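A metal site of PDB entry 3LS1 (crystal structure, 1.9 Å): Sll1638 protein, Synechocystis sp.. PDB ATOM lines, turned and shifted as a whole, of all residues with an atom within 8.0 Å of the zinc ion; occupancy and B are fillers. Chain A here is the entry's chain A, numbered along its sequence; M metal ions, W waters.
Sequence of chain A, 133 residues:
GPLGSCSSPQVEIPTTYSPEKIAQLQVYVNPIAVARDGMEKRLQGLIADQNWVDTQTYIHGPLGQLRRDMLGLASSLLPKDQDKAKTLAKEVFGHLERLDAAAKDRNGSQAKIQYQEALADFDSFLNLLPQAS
Water W1 lies within hydrogen-bond range of O of Glu 117 (2.9 Å) and OD1 of Asp 121 (3.2 Å).
The side-chain carboxylate (OE1) of Glu 117 lies within hydrogen-bond range of a ring nitrogen (ND1) of His 95 (3.3 Å).
OE1 of Gln 114 is in hydrogen-bond range of ND1 of His 95, at 2.9 Å.
A ring nitrogen (NE2) of His 95 is bound to the zinc ion (1.8 Å).
The zinc ion is bound by the side-chain carboxylate (OE1) of Glu 91 (1.9 Å).
OD2 of Asp 121 is bound to the zinc ion (2.0 Å).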
ATOM      1  N   THR A  87      12.812  11.229  10.030  1.00  0.00           N
ATOM      2  CA  THR A  87      12.908  10.887   8.589  1.00  0.00           C
ATOM      3  C   THR A  87      11.611  11.305   7.837  1.00  0.00           C
ATOM      4  O   THR A  87      11.664  11.819   6.708  1.00  0.00           O
ATOM      5  CB  THR A  87      13.144   9.413   8.491  1.00  0.00           C
ATOM      6  OG1 THR A  87      14.432   9.105   9.013  1.00  0.00           O
ATOM      7  CG2 THR A  87      13.053   8.967   6.995  1.00  0.00           C
ATOM      8  N   LEU A  88      10.458  11.025   8.449  1.00  0.00           N
ATOM      9  CA  LEU A  88       9.178  11.462   7.875  1.00  0.00           C
ATOM     10  C   LEU A  88       9.009  13.000   7.734  1.00  0.00           C
ATOM     11  O   LEU A  88       8.435  13.474   6.756  1.00  0.00           O
ATOM     12  CB  LEU A  88       7.982  10.822   8.620  1.00  0.00           C
ATOM     13  CG  LEU A  88       7.826   9.292   8.301  1.00  0.00           C
ATOM     14  CD1 LEU A  88       6.873   8.583   9.320  1.00  0.00           C
ATOM     15  CD2 LEU A  88       7.288   9.011   6.828  1.00  0.00           C
ATOM     16  N   LYS A  90      11.411  14.998   7.182  1.00  0.00           N
ATOM     17  CA  LYS A  90      12.305  15.397   6.048  1.00  0.00           C
ATOM     18  C   LYS A  90      11.658  14.999   4.703  1.00  0.00           C
ATOM     19  O   LYS A  90      11.770  15.723   3.690  1.00  0.00           O
ATOM     20  CB  LYS A  90      13.657  14.735   6.217  1.00  0.00           C
ATOM     21  CG  LYS A  90      14.432  15.378   7.347  1.00  0.00           C
ATOM     22  CD  LYS A  90      15.829  14.740   7.512  1.00  0.00           C
ATOM     23  CE  LYS A  90      16.566  15.516   8.571  1.00  0.00           C
ATOM     24  NZ  LYS A  90      17.915  14.924   8.863  1.00  0.00           N
ATOM     25  N   GLU A  91      10.977  13.849   4.730  1.00  0.00           N
ATOM     26  CA  GLU A  91      10.219  13.390   3.504  1.00  0.00           C
ATOM     27  C   GLU A  91       9.130  14.335   3.161  1.00  0.00           C
ATOM     28  O   GLU A  91       8.959  14.680   2.001  1.00  0.00           O
ATOM     29  CB  GLU A  91       9.577  12.031   3.804  1.00  0.00           C
ATOM     30  CG  GLU A  91      10.380  10.896   3.528  1.00  0.00           C
ATOM     31  CD  GLU A  91      10.703  10.804   2.013  1.00  0.00           C
ATOM     32  OE1 GLU A  91       9.768  10.588   1.123  1.00  0.00           O
ATOM     33  OE2 GLU A  91      11.928  10.908   1.790  1.00  0.00           O
ATOM     34  N   VAL A  92       8.368  14.834   4.157  1.00  0.00           N
ATOM     35  CA  VAL A  92       7.277  15.774   3.830  1.00  0.00           C
ATOM     36  C   VAL A  92       7.893  17.030   3.188  1.00  0.00           C
ATOM     37  O   VAL A  92       7.406  17.559   2.171  1.00  0.00           O
ATOM     38  CB  VAL A  92       6.434  16.104   5.112  1.00  0.00           C
ATOM     39  CG1 VAL A  92       5.536  17.319   4.896  1.00  0.00           C
ATOM     40  CG2 VAL A  92       5.548  14.886   5.517  1.00  0.00           C
ATOM     41  N   PHE A  93       8.962  17.587   3.812  1.00  0.00           N
ATOM     42  CA  PHE A  93       9.611  18.764   3.274  1.00  0.00           C
ATOM     43  C   PHE A  93      10.023  18.493   1.793  1.00  0.00           C
ATOM     44  O   PHE A  93       9.822  19.319   0.899  1.00  0.00           O
ATOM     45  CB  PHE A  93      10.840  18.982   4.089  1.00  0.00           C
ATOM     46  CG  PHE A  93      11.670  20.161   3.648  1.00  0.00           C
ATOM     47  CD1 PHE A  93      11.234  21.462   3.876  1.00  0.00           C
ATOM     48  CD2 PHE A  93      12.856  19.963   2.947  1.00  0.00           C
ATOM     49  CE1 PHE A  93      12.076  22.609   3.500  1.00  0.00           C
ATOM     50  CE2 PHE A  93      13.643  21.053   2.511  1.00  0.00           C
ATOM     51  CZ  PHE A  93      13.276  22.397   2.785  1.00  0.00           C
ATOM     52  N   GLY A  94      10.663  17.356   1.572  1.00  0.00           N
ATOM     53  CA  GLY A  94      11.067  16.965   0.213  1.00  0.00           C
ATOM     54  C   GLY A  94       9.944  16.988  -0.816  1.00  0.00           C
ATOM     55  O   GLY A  94      10.157  17.472  -1.938  1.00  0.00           O
ATOM     56  N   HIS A  95       8.809  16.373  -0.460  1.00  0.00           N
ATOM     57  CA  HIS A  95       7.675  16.438  -1.370  1.00  0.00           C
ATOM     58  C   HIS A  95       7.133  17.870  -1.561  1.00  0.00           C
ATOM     59  O   HIS A  95       6.638  18.184  -2.586  1.00  0.00           O
ATOM     60  CB  HIS A  95       6.542  15.420  -0.984  1.00  0.00           C
ATOM     61  CG  HIS A  95       7.000  13.962  -0.879  1.00  0.00           C
ATOM     62  ND1 HIS A  95       7.413  13.212  -1.988  1.00  0.00           N
ATOM     63  CD2 HIS A  95       7.058  13.128   0.193  1.00  0.00           C
ATOM     64  CE1 HIS A  95       7.724  11.979  -1.584  1.00  0.00           C
ATOM     65  NE2 HIS A  95       7.501  11.849  -0.271  1.00  0.00           N
ATOM     66  N   ARG A  98       9.246  19.430  -4.063  1.00  0.00           N
ATOM     67  CA  ARG A  98       8.965  18.839  -5.426  1.00  0.00           C
ATOM     68  C   ARG A  98       7.635  19.431  -5.897  1.00  0.00           C
ATOM     69  O   ARG A  98       7.476  19.767  -7.100  1.00  0.00           O
ATOM     70  CB  ARG A  98       8.938  17.313  -5.370  1.00  0.00           C
ATOM     71  CG  ARG A  98      10.224  16.680  -5.613  1.00  0.00           C
ATOM     72  CD  ARG A  98      10.935  16.051  -4.491  1.00  0.00           C
ATOM     73  NE  ARG A  98      10.561  14.668  -4.247  1.00  0.00           N
ATOM     74  CZ  ARG A  98      11.156  13.856  -3.357  1.00  0.00           C
ATOM     75  NH1 ARG A  98      12.227  14.260  -2.661  1.00  0.00           N
ATOM     76  NH2 ARG A  98      10.721  12.628  -3.228  1.00  0.00           N
ATOM     77  N   GLN A 114       2.771  14.858  -5.899  1.00  0.00           N
ATOM     78  CA  GLN A 114       3.606  15.241  -4.775  1.00  0.00           C
ATOM     79  C   GLN A 114       2.730  15.631  -3.595  1.00  0.00           C
ATOM     80  O   GLN A 114       3.131  15.437  -2.415  1.00  0.00           O
ATOM     81  CB  GLN A 114       4.486  16.438  -5.137  1.00  0.00           C
ATOM     82  CG  GLN A 114       5.602  16.069  -6.091  1.00  0.00           C
ATOM     83  CD  GLN A 114       6.452  14.911  -5.538  1.00  0.00           C
ATOM     84  OE1 GLN A 114       6.776  14.869  -4.343  1.00  0.00           O
ATOM     85  NE2 GLN A 114       6.917  14.090  -6.406  1.00  0.00           N
ATOM     86  N   GLN A 116      -0.073  14.220  -2.778  1.00  0.00           N
ATOM     87  CA  GLN A 116      -0.475  12.935  -2.152  1.00  0.00           C
ATOM     88  C   GLN A 116       0.666  12.305  -1.366  1.00  0.00           C
ATOM     89  O   GLN A 116       0.460  11.748  -0.300  1.00  0.00           O
ATOM     90  CB  GLN A 116      -0.821  11.926  -3.286  1.00  0.00           C
ATOM     91  CG  GLN A 116      -2.183  12.108  -3.672  1.00  0.00           C
ATOM     92  CD  GLN A 116      -2.537  11.454  -5.003  1.00  0.00           C
ATOM     93  OE1 GLN A 116      -3.593  11.776  -5.550  1.00  0.00           O
ATOM     94  NE2 GLN A 116      -1.669  10.589  -5.545  1.00  0.00           N
ATOM     95  N   GLU A 117       1.838  12.289  -1.957  1.00  0.00           N
ATOM     96  CA  GLU A 117       3.004  11.679  -1.314  1.00  0.00           C
ATOM     97  C   GLU A 117       3.337  12.495  -0.001  1.00  0.00           C
ATOM     98  O   GLU A 117       3.754  11.867   1.002  1.00  0.00           O
ATOM     99  CB  GLU A 117       4.207  11.751  -2.245  1.00  0.00           C
ATOM    100  CG  GLU A 117       4.038  10.591  -3.338  1.00  0.00           C
ATOM    101  CD  GLU A 117       5.257  10.471  -4.279  1.00  0.00           C
ATOM    102  OE1 GLU A 117       6.079  11.379  -4.387  1.00  0.00           O
ATOM    103  OE2 GLU A 117       5.312   9.420  -4.947  1.00  0.00           O
ATOM    104  N   ALA A 118       3.326  13.831  -0.099  1.00  0.00           N
ATOM    105  CA  ALA A 118       3.509  14.659   1.095  1.00  0.00           C
ATOM    106  C   ALA A 118       2.430  14.271   2.170  1.00  0.00           C
ATOM    107  O   ALA A 118       2.798  14.060   3.310  1.00  0.00           O
ATOM    108  CB  ALA A 118       3.387  16.132   0.803  1.00  0.00           C
ATOM    109  N   LEU A 119       1.145  14.168   1.786  1.00  0.00           N
ATOM    110  CA  LEU A 119       0.159  13.756   2.782  1.00  0.00           C
ATOM    111  C   LEU A 119       0.356  12.376   3.286  1.00  0.00           C
ATOM    112  O   LEU A 119       0.079  12.160   4.447  1.00  0.00           O
ATOM    113  CB  LEU A 119      -1.249  13.926   2.223  1.00  0.00           C
ATOM    114  CG  LEU A 119      -1.977  15.258   2.154  1.00  0.00           C
ATOM    115  CD1 LEU A 119      -3.435  14.979   1.811  1.00  0.00           C
ATOM    116  CD2 LEU A 119      -1.808  16.011   3.548  1.00  0.00           C
ATOM    117  N   ALA A 120       0.757  11.392   2.442  1.00  0.00           N
ATOM    118  CA  ALA A 120       0.963  10.028   2.934  1.00  0.00           C
ATOM    119  C   ALA A 120       2.086  10.015   4.032  1.00  0.00           C
ATOM    120  O   ALA A 120       1.955   9.315   5.038  1.00  0.00           O
ATOM    121  CB  ALA A 120       1.398   9.037   1.789  1.00  0.00           C
ATOM    122  N   ASP A 121       3.187  10.683   3.760  1.00  0.00           N
ATOM    123  CA  ASP A 121       4.278  10.673   4.765  1.00  0.00           C
ATOM    124  C   ASP A 121       3.867  11.527   5.995  1.00  0.00           C
ATOM    125  O   ASP A 121       4.244  11.171   7.149  1.00  0.00           O
ATOM    126  CB  ASP A 121       5.570  11.255   4.264  1.00  0.00           C
ATOM    127  CG  ASP A 121       6.192  10.374   3.182  1.00  0.00           C
ATOM    128  OD1 ASP A 121       5.942   9.180   3.152  1.00  0.00           O
ATOM    129  OD2 ASP A 121       6.922  10.951   2.410  1.00  0.00           O
ATOM    130  N   PHE A 122       3.074  12.557   5.728  1.00  0.00           N
ATOM    131  CA  PHE A 122       2.580  13.393   6.917  1.00  0.00           C
ATOM    132  C   PHE A 122       1.692  12.516   7.818  1.00  0.00           C
ATOM    133  O   PHE A 122       1.816  12.509   9.038  1.00  0.00           O
ATOM    134  CB  PHE A 122       1.760  14.527   6.398  1.00  0.00           C
ATOM    135  CG  PHE A 122       1.642  15.743   7.353  1.00  0.00           C
ATOM    136  CD1 PHE A 122       1.799  15.605   8.769  1.00  0.00           C
ATOM    137  CD2 PHE A 122       1.305  16.993   6.805  1.00  0.00           C
ATOM    138  CE1 PHE A 122       1.646  16.750   9.548  1.00  0.00           C
ATOM    139  CE2 PHE A 122       1.102  18.143   7.590  1.00  0.00           C
ATOM    140  CZ  PHE A 122       1.295  17.995   8.991  1.00  0.00           C
HETATM  141 ZN    ZN M   1       7.944  10.405   0.721  1.00  0.00          ZN
HETATM  142  O   HOH W   1       4.810   9.277   0.187  1.00  0.00           O
